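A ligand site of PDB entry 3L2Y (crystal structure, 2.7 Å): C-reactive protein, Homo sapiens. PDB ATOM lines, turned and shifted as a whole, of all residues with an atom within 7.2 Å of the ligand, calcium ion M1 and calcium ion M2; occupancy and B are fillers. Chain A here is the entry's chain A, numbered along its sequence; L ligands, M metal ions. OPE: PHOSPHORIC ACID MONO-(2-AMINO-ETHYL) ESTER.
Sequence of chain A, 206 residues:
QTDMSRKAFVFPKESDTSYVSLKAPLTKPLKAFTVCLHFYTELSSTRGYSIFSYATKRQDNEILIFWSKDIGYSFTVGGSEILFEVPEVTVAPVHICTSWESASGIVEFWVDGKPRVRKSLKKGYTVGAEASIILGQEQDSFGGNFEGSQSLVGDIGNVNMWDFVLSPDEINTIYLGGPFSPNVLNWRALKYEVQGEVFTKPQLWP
Of the 22 residues printed, 5 come within 4 Å of calcium ion M1. The nearest printed residue that does not touch calcium ion M1 is Leu 64 (5.3 Å).
Calcium ion M2 is bound by an oxygen (O2) of the ligand (2.3 Å), the side-chain carboxylate (OD1) of Asp 140 (2.5 Å), the side-chain carboxylate (OE1) of Glu 138 (2.6 Å), the side-chain carboxylate (OE2) of Glu 147 (2.6 Å), the side-chain carboxylate (OD2) of Asp 140 (2.6 Å) and the side-chain amide oxygen (OE1) of Gln 150 (2.6 Å). Calcium ion M2 has six donor atoms within binding distance.
Of the 22 residues printed, 4 come within 4 Å of calcium ion M2. The nearest printed residue that does not touch calcium ion M2 is Gln 139 (4.8 Å).
O1 of the ligand binds calcium ion M1, 2.4 Å away. O of Gln 139 is bound to calcium ion M1. Calcium ion M1 is bound by OD1 of Asn 61, at 2.5 Å. Calcium ion M1 is bound by OE1 of Glu 138 (2.6 Å). Calcium ion M1 is bound by the side-chain carboxylate (OD1) of Asp 140, at 2.6 Å. The side-chain carboxylate (OE2) of Glu 138 is bound to calcium ion M1. Calcium ion M1 is bound by OD2 of Asp 60, at 2.7 Å. Calcium ion M1 has seven donor atoms within binding distance.
N of the ligand is in salt-bridge range of OE2 of Glu 81 (3.7 Å).
O of Asn 145 sits close to N of Asp 140, 3.3 Å away. The side-chain carboxylate (OD1) of Asp 60 lies close to the side-chain amide oxygen (OE1) of Gln 59. The backbone NH (N) of Asn 61 lies within hydrogen-bond range of the side-chain amide oxygen (OE1) of Gln 59, 3.1 Å away. The backbone carbonyl oxygen (O) of Gln 150 sits at hydrogen-bond distance from the backbone NH (N) of Ser 50 (2.9 Å). The backbone NH of Leu 64 sits at hydrogen-bond distance from the backbone carbonyl oxygen of Thr 76 (2.8 Å). O of Phe 66 sits at hydrogen-bond distance from N of Ser 74 (2.7 Å). OE2 of Glu 81 sits at hydrogen-bond distance from OG of Ser 74 (3.0 Å). The side-chain amide nitrogen (NE2) of Gln 139 sits at hydrogen-bond distance from the side-chain hydroxyl (OG) of Ser 53 (3.0 Å).
Merely in contact with the ligand: Leu 64 and Phe 66. Hydrophobic or aromatic side chains that line the ligand: Leu 64 and Phe 66. Within 4 Å of the ligand: Asn 61, Leu 64, Phe 66, Glu 81, Glu 138, Asp 140, Glu 147 and Gln 150. The nearest printed residue that does not touch the ligand is Asp 60 (4.05 Å).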
ATOM      1  N   TYR A  49      25.798  22.206 -12.906  1.00  0.00           N
ATOM      2  CA  TYR A  49      25.357  23.142 -11.880  1.00  0.00           C
ATOM      3  C   TYR A  49      26.444  24.128 -11.471  1.00  0.00           C
ATOM      4  O   TYR A  49      27.639  23.835 -11.604  1.00  0.00           O
ATOM      5  CB  TYR A  49      24.850  22.418 -10.633  1.00  0.00           C
ATOM      6  CG  TYR A  49      25.817  21.419 -10.065  1.00  0.00           C
ATOM      7  CD1 TYR A  49      26.714  21.776  -9.078  1.00  0.00           C
ATOM      8  CD2 TYR A  49      25.810  20.109 -10.500  1.00  0.00           C
ATOM      9  CE1 TYR A  49      27.597  20.845  -8.546  1.00  0.00           C
ATOM     10  CE2 TYR A  49      26.681  19.182  -9.980  1.00  0.00           C
ATOM     11  CZ  TYR A  49      27.583  19.554  -9.011  1.00  0.00           C
ATOM     12  OH  TYR A  49      28.454  18.610  -8.506  1.00  0.00           O
ATOM     13  N   SER A  50      26.019  25.301 -10.986  1.00  0.00           N
ATOM     14  CA  SER A  50      26.936  26.327 -10.510  1.00  0.00           C
ATOM     15  C   SER A  50      27.252  26.157  -9.023  1.00  0.00           C
ATOM     16  O   SER A  50      26.356  26.059  -8.179  1.00  0.00           O
ATOM     17  CB  SER A  50      26.362  27.724 -10.780  1.00  0.00           C
ATOM     18  OG  SER A  50      27.016  28.700  -9.994  1.00  0.00           O
ATOM     19  N   SER A  53      29.266  31.553  -8.144  1.00  0.00           N
ATOM     20  CA  SER A  53      29.146  32.519  -9.245  1.00  0.00           C
ATOM     21  C   SER A  53      29.490  33.948  -8.836  1.00  0.00           C
ATOM     22  O   SER A  53      28.835  34.532  -7.974  1.00  0.00           O
ATOM     23  CB  SER A  53      27.736  32.512  -9.854  1.00  0.00           C
ATOM     24  OG  SER A  53      27.668  33.378 -10.980  1.00  0.00           O
ATOM     25  N   GLN A  59      31.296  41.389 -16.847  1.00  0.00           N
ATOM     26  CA  GLN A  59      31.513  39.959 -17.067  1.00  0.00           C
ATOM     27  C   GLN A  59      30.696  39.116 -16.089  1.00  0.00           C
ATOM     28  O   GLN A  59      30.910  39.164 -14.877  1.00  0.00           O
ATOM     29  CB  GLN A  59      33.006  39.634 -16.940  1.00  0.00           C
ATOM     30  CG  GLN A  59      33.320  38.164 -16.984  1.00  0.00           C
ATOM     31  CD  GLN A  59      33.066  37.564 -18.336  1.00  0.00           C
ATOM     32  OE1 GLN A  59      32.177  36.738 -18.509  1.00  0.00           O
ATOM     33  NE2 GLN A  59      33.860  37.980 -19.323  1.00  0.00           N
ATOM     34  N   ASP A  60      29.759  38.335 -16.628  1.00  0.00           N
ATOM     35  CA  ASP A  60      28.906  37.489 -15.800  1.00  0.00           C
ATOM     36  C   ASP A  60      29.670  36.323 -15.171  1.00  0.00           C
ATOM     37  O   ASP A  60      29.301  35.829 -14.118  1.00  0.00           O
ATOM     38  CB  ASP A  60      27.694  36.996 -16.602  1.00  0.00           C
ATOM     39  CG  ASP A  60      28.077  36.161 -17.832  1.00  0.00           C
ATOM     40  OD1 ASP A  60      29.086  36.466 -18.499  1.00  0.00           O
ATOM     41  OD2 ASP A  60      27.343  35.207 -18.142  1.00  0.00           O
ATOM     42  N   ASN A  61      30.760  35.924 -15.820  1.00  0.00           N
ATOM     43  CA  ASN A  61      31.588  34.844 -15.330  1.00  0.00           C
ATOM     44  C   ASN A  61      32.976  35.317 -14.965  1.00  0.00           C
ATOM     45  O   ASN A  61      33.971  34.815 -15.499  1.00  0.00           O
ATOM     46  CB  ASN A  61      31.644  33.737 -16.380  1.00  0.00           C
ATOM     47  CG  ASN A  61      30.262  33.185 -16.700  1.00  0.00           C
ATOM     48  OD1 ASN A  61      29.275  33.602 -16.108  1.00  0.00           O
ATOM     49  ND2 ASN A  61      30.196  32.252 -17.623  1.00  0.00           N
ATOM     50  N   LEU A  64      34.011  31.773 -11.876  1.00  0.00           N
ATOM     51  CA  LEU A  64      32.955  30.759 -11.871  1.00  0.00           C
ATOM     52  C   LEU A  64      33.476  29.356 -11.617  1.00  0.00           C
ATOM     53  O   LEU A  64      34.255  28.819 -12.397  1.00  0.00           O
ATOM     54  CB  LEU A  64      32.154  30.771 -13.176  1.00  0.00           C
ATOM     55  CG  LEU A  64      31.070  29.702 -13.211  1.00  0.00           C
ATOM     56  CD1 LEU A  64      30.003  29.978 -12.161  1.00  0.00           C
ATOM     57  CD2 LEU A  64      30.432  29.581 -14.587  1.00  0.00           C
ATOM     58  N   PHE A  66      32.089  25.676 -11.484  1.00  0.00           N
ATOM     59  CA  PHE A  66      30.920  25.049 -12.077  1.00  0.00           C
ATOM     60  C   PHE A  66      31.183  23.567 -12.310  1.00  0.00           C
ATOM     61  O   PHE A  66      32.318  23.161 -12.576  1.00  0.00           O
ATOM     62  CB  PHE A  66      30.662  25.727 -13.406  1.00  0.00           C
ATOM     63  CG  PHE A  66      29.371  25.353 -14.048  1.00  0.00           C
ATOM     64  CD1 PHE A  66      28.229  26.093 -13.795  1.00  0.00           C
ATOM     65  CD2 PHE A  66      29.303  24.306 -14.954  1.00  0.00           C
ATOM     66  CE1 PHE A  66      27.023  25.779 -14.413  1.00  0.00           C
ATOM     67  CE2 PHE A  66      28.099  23.983 -15.568  1.00  0.00           C
ATOM     68  CZ  PHE A  66      26.970  24.723 -15.294  1.00  0.00           C
ATOM     69  N   TRP A  67      30.155  22.743 -12.181  1.00  0.00           N
ATOM     70  CA  TRP A  67      30.295  21.337 -12.517  1.00  0.00           C
ATOM     71  C   TRP A  67      29.584  21.131 -13.830  1.00  0.00           C
ATOM     72  O   TRP A  67      28.380  21.366 -13.934  1.00  0.00           O
ATOM     73  CB  TRP A  67      29.648  20.443 -11.450  1.00  0.00           C
ATOM     74  CG  TRP A  67      29.649  19.007 -11.874  1.00  0.00           C
ATOM     75  CD1 TRP A  67      28.681  18.361 -12.601  1.00  0.00           C
ATOM     76  CD2 TRP A  67      30.666  18.045 -11.631  1.00  0.00           C
ATOM     77  NE1 TRP A  67      29.045  17.049 -12.815  1.00  0.00           N
ATOM     78  CE2 TRP A  67      30.260  16.833 -12.229  1.00  0.00           C
ATOM     79  CE3 TRP A  67      31.887  18.077 -10.957  1.00  0.00           C
ATOM     80  CZ2 TRP A  67      31.027  15.688 -12.176  1.00  0.00           C
ATOM     81  CZ3 TRP A  67      32.643  16.940 -10.907  1.00  0.00           C
ATOM     82  CH2 TRP A  67      32.222  15.753 -11.515  1.00  0.00           C
ATOM     83  N   SER A  68      30.320  20.704 -14.852  1.00  0.00           N
ATOM     84  CA  SER A  68      29.672  20.436 -16.131  1.00  0.00           C
ATOM     85  C   SER A  68      29.502  18.924 -16.371  1.00  0.00           C
ATOM     86  O   SER A  68      30.425  18.139 -16.112  1.00  0.00           O
ATOM     87  CB  SER A  68      30.372  21.167 -17.293  1.00  0.00           C
ATOM     88  OG  SER A  68      31.592  20.550 -17.603  1.00  0.00           O
ATOM     89  N   SER A  74      34.615  22.825 -13.874  1.00  0.00           N
ATOM     90  CA  SER A  74      34.969  23.888 -14.802  1.00  0.00           C
ATOM     91  C   SER A  74      35.297  25.151 -14.025  1.00  0.00           C
ATOM     92  O   SER A  74      34.515  25.610 -13.190  1.00  0.00           O
ATOM     93  CB  SER A  74      33.826  24.140 -15.778  1.00  0.00           C
ATOM     94  OG  SER A  74      33.549  25.528 -15.864  1.00  0.00           O
ATOM     95  N   THR A  76      36.337  29.151 -14.311  1.00  0.00           N
ATOM     96  CA  THR A  76      36.339  30.275 -15.225  1.00  0.00           C
ATOM     97  C   THR A  76      36.802  31.572 -14.558  1.00  0.00           C
ATOM     98  O   THR A  76      36.311  31.951 -13.496  1.00  0.00           O
ATOM     99  CB  THR A  76      34.938  30.494 -15.824  1.00  0.00           C
ATOM    100  OG1 THR A  76      34.441  29.256 -16.363  1.00  0.00           O
ATOM    101  CG2 THR A  76      34.990  31.554 -16.909  1.00  0.00           C
ATOM    102  N   GLU A  81      37.609  29.657 -19.718  1.00  0.00           N
ATOM    103  CA  GLU A  81      37.325  28.432 -18.996  1.00  0.00           C
ATOM    104  C   GLU A  81      38.446  27.420 -19.152  1.00  0.00           C
ATOM    105  O   GLU A  81      38.984  27.257 -20.245  1.00  0.00           O
ATOM    106  CB  GLU A  81      36.009  27.830 -19.516  1.00  0.00           C
ATOM    107  CG  GLU A  81      35.574  26.531 -18.874  1.00  0.00           C
ATOM    108  CD  GLU A  81      34.365  25.904 -19.553  1.00  0.00           C
ATOM    109  OE1 GLU A  81      34.421  25.731 -20.790  1.00  0.00           O
ATOM    110  OE2 GLU A  81      33.359  25.598 -18.864  1.00  0.00           O
ATOM    111  N   GLU A 138      23.398  30.332 -11.187  1.00  0.00           N
ATOM    112  CA  GLU A 138      24.476  30.773 -12.058  1.00  0.00           C
ATOM    113  C   GLU A 138      24.035  32.081 -12.701  1.00  0.00           C
ATOM    114  O   GLU A 138      22.960  32.167 -13.292  1.00  0.00           O
ATOM    115  CB  GLU A 138      24.785  29.727 -13.127  1.00  0.00           C
ATOM    116  CG  GLU A 138      26.201  29.797 -13.724  1.00  0.00           C
ATOM    117  CD  GLU A 138      26.416  31.015 -14.614  1.00  0.00           C
ATOM    118  OE1 GLU A 138      25.573  31.229 -15.502  1.00  0.00           O
ATOM    119  OE2 GLU A 138      27.411  31.763 -14.413  1.00  0.00           O
ATOM    120  N   GLN A 139      24.862  33.117 -12.551  1.00  0.00           N
ATOM    121  CA  GLN A 139      24.545  34.452 -13.059  1.00  0.00           C
ATOM    122  C   GLN A 139      24.861  34.614 -14.533  1.00  0.00           C
ATOM    123  O   GLN A 139      25.964  34.293 -14.976  1.00  0.00           O
ATOM    124  CB  GLN A 139      25.340  35.492 -12.287  1.00  0.00           C
ATOM    125  CG  GLN A 139      24.804  35.795 -10.917  1.00  0.00           C
ATOM    126  CD  GLN A 139      25.763  36.638 -10.111  1.00  0.00           C
ATOM    127  OE1 GLN A 139      25.443  37.774  -9.736  1.00  0.00           O
ATOM    128  NE2 GLN A 139      26.955  36.098  -9.864  1.00  0.00           N
ATOM    129  N   ASP A 140      23.900  35.124 -15.292  1.00  0.00           N
ATOM    130  CA  ASP A 140      24.156  35.503 -16.671  1.00  0.00           C
ATOM    131  C   ASP A 140      24.170  37.020 -16.818  1.00  0.00           C
ATOM    132  O   ASP A 140      24.492  37.562 -17.867  1.00  0.00           O
ATOM    133  CB  ASP A 140      23.108  34.901 -17.598  1.00  0.00           C
ATOM    134  CG  ASP A 140      23.428  33.480 -17.970  1.00  0.00           C
ATOM    135  OD1 ASP A 140      24.602  33.083 -17.794  1.00  0.00           O
ATOM    136  OD2 ASP A 140      22.529  32.764 -18.451  1.00  0.00           O
ATOM    137  N   SER A 141      23.820  37.711 -15.735  1.00  0.00           N
ATOM    138  CA  SER A 141      23.886  39.151 -15.698  1.00  0.00           C
ATOM    139  C   SER A 141      24.258  39.532 -14.289  1.00  0.00           C
ATOM    140  O   SER A 141      24.173  38.710 -13.382  1.00  0.00           O
ATOM    141  CB  SER A 141      22.538  39.760 -16.076  1.00  0.00           C
ATOM    142  OG  SER A 141      21.618  39.653 -15.009  1.00  0.00           O
ATOM    143  N   GLY A 144      21.629  38.545 -11.570  1.00  0.00           N
ATOM    144  CA  GLY A 144      20.439  37.875 -12.046  1.00  0.00           C
ATOM    145  C   GLY A 144      20.566  37.078 -13.332  1.00  0.00           C
ATOM    146  O   GLY A 144      21.668  36.654 -13.731  1.00  0.00           O
ATOM    147  N   ASN A 145      19.422  36.883 -13.983  1.00  0.00           N
ATOM    148  CA  ASN A 145      19.347  36.071 -15.188  1.00  0.00           C
ATOM    149  C   ASN A 145      19.809  34.655 -14.936  1.00  0.00           C
ATOM    150  O   ASN A 145      20.749  34.176 -15.575  1.00  0.00           O
ATOM    151  CB  ASN A 145      20.125  36.690 -16.338  1.00  0.00           C
ATOM    152  CG  ASN A 145      19.307  37.710 -17.076  1.00  0.00           C
ATOM    153  OD1 ASN A 145      19.682  38.886 -17.149  1.00  0.00           O
ATOM    154  ND2 ASN A 145      18.177  37.292 -17.610  1.00  0.00           N
ATOM    155  N   PHE A 146      19.134  33.993 -14.012  1.00  0.00           N
ATOM    156  CA  PHE A 146      19.482  32.643 -13.608  1.00  0.00           C
ATOM    157  C   PHE A 146      18.876  31.626 -14.564  1.00  0.00           C
ATOM    158  O   PHE A 146      17.844  31.891 -15.170  1.00  0.00           O
ATOM    159  CB  PHE A 146      18.967  32.395 -12.196  1.00  0.00           C
ATOM    160  CG  PHE A 146      19.376  33.460 -11.218  1.00  0.00           C
ATOM    161  CD1 PHE A 146      20.703  33.861 -11.124  1.00  0.00           C
ATOM    162  CD2 PHE A 146      18.449  34.074 -10.398  1.00  0.00           C
ATOM    163  CE1 PHE A 146      21.074  34.842 -10.227  1.00  0.00           C
ATOM    164  CE2 PHE A 146      18.822  35.045  -9.497  1.00  0.00           C
ATOM    165  CZ  PHE A 146      20.140  35.431  -9.407  1.00  0.00           C
ATOM    166  N   GLU A 147      19.529  30.475 -14.710  1.00  0.00           N
ATOM    167  CA  GLU A 147      18.973  29.351 -15.448  1.00  0.00           C
ATOM    168  C   GLU A 147      18.746  28.225 -14.466  1.00  0.00           C
ATOM    169  O   GLU A 147      19.648  27.843 -13.716  1.00  0.00           O
ATOM    170  CB  GLU A 147      19.921  28.864 -16.553  1.00  0.00           C
ATOM    171  CG  GLU A 147      20.307  29.868 -17.632  1.00  0.00           C
ATOM    172  CD  GLU A 147      21.057  29.214 -18.807  1.00  0.00           C
ATOM    173  OE1 GLU A 147      20.451  28.351 -19.480  1.00  0.00           O
ATOM    174  OE2 GLU A 147      22.241  29.551 -19.060  1.00  0.00           O
ATOM    175  N   GLN A 150      20.840  25.118 -14.200  1.00  0.00           N
ATOM    176  CA  GLN A 150      22.193  25.305 -13.688  1.00  0.00           C
ATOM    177  C   GLN A 150      22.216  25.570 -12.189  1.00  0.00           C
ATOM    178  O   GLN A 150      23.265  25.867 -11.620  1.00  0.00           O
ATOM    179  CB  GLN A 150      22.892  26.442 -14.437  1.00  0.00           C
ATOM    180  CG  GLN A 150      23.204  26.091 -15.873  1.00  0.00           C
ATOM    181  CD  GLN A 150      23.966  27.184 -16.574  1.00  0.00           C
ATOM    182  OE1 GLN A 150      23.825  28.335 -16.215  1.00  0.00           O
ATOM    183  NE2 GLN A 150      24.789  26.825 -17.553  1.00  0.00           N
HETATM  184  CA  OPE L   1      28.757  28.646 -17.759  1.00  0.00           C
HETATM  185  CB  OPE L   1      29.222  27.312 -17.292  1.00  0.00           C
HETATM  186  O1  OPE L   1      27.721  31.178 -18.192  1.00  0.00           O
HETATM  187  O2  OPE L   1      25.556  30.334 -18.616  1.00  0.00           O
HETATM  188  O3  OPE L   1      27.295  30.254 -20.388  1.00  0.00           O
HETATM  189  O4  OPE L   1      27.448  28.758 -18.316  1.00  0.00           O
HETATM  190  N   OPE L   1      29.845  26.416 -18.279  1.00  0.00           N
HETATM  191  P   OPE L   1      26.999  30.137 -18.946  1.00  0.00           P
HETATM  192 CA    CA M   1      26.986  32.951 -16.751  1.00  0.00          CA
HETATM  193 CA    CA M   2      23.770  30.749 -17.282  1.00  0.00          CA
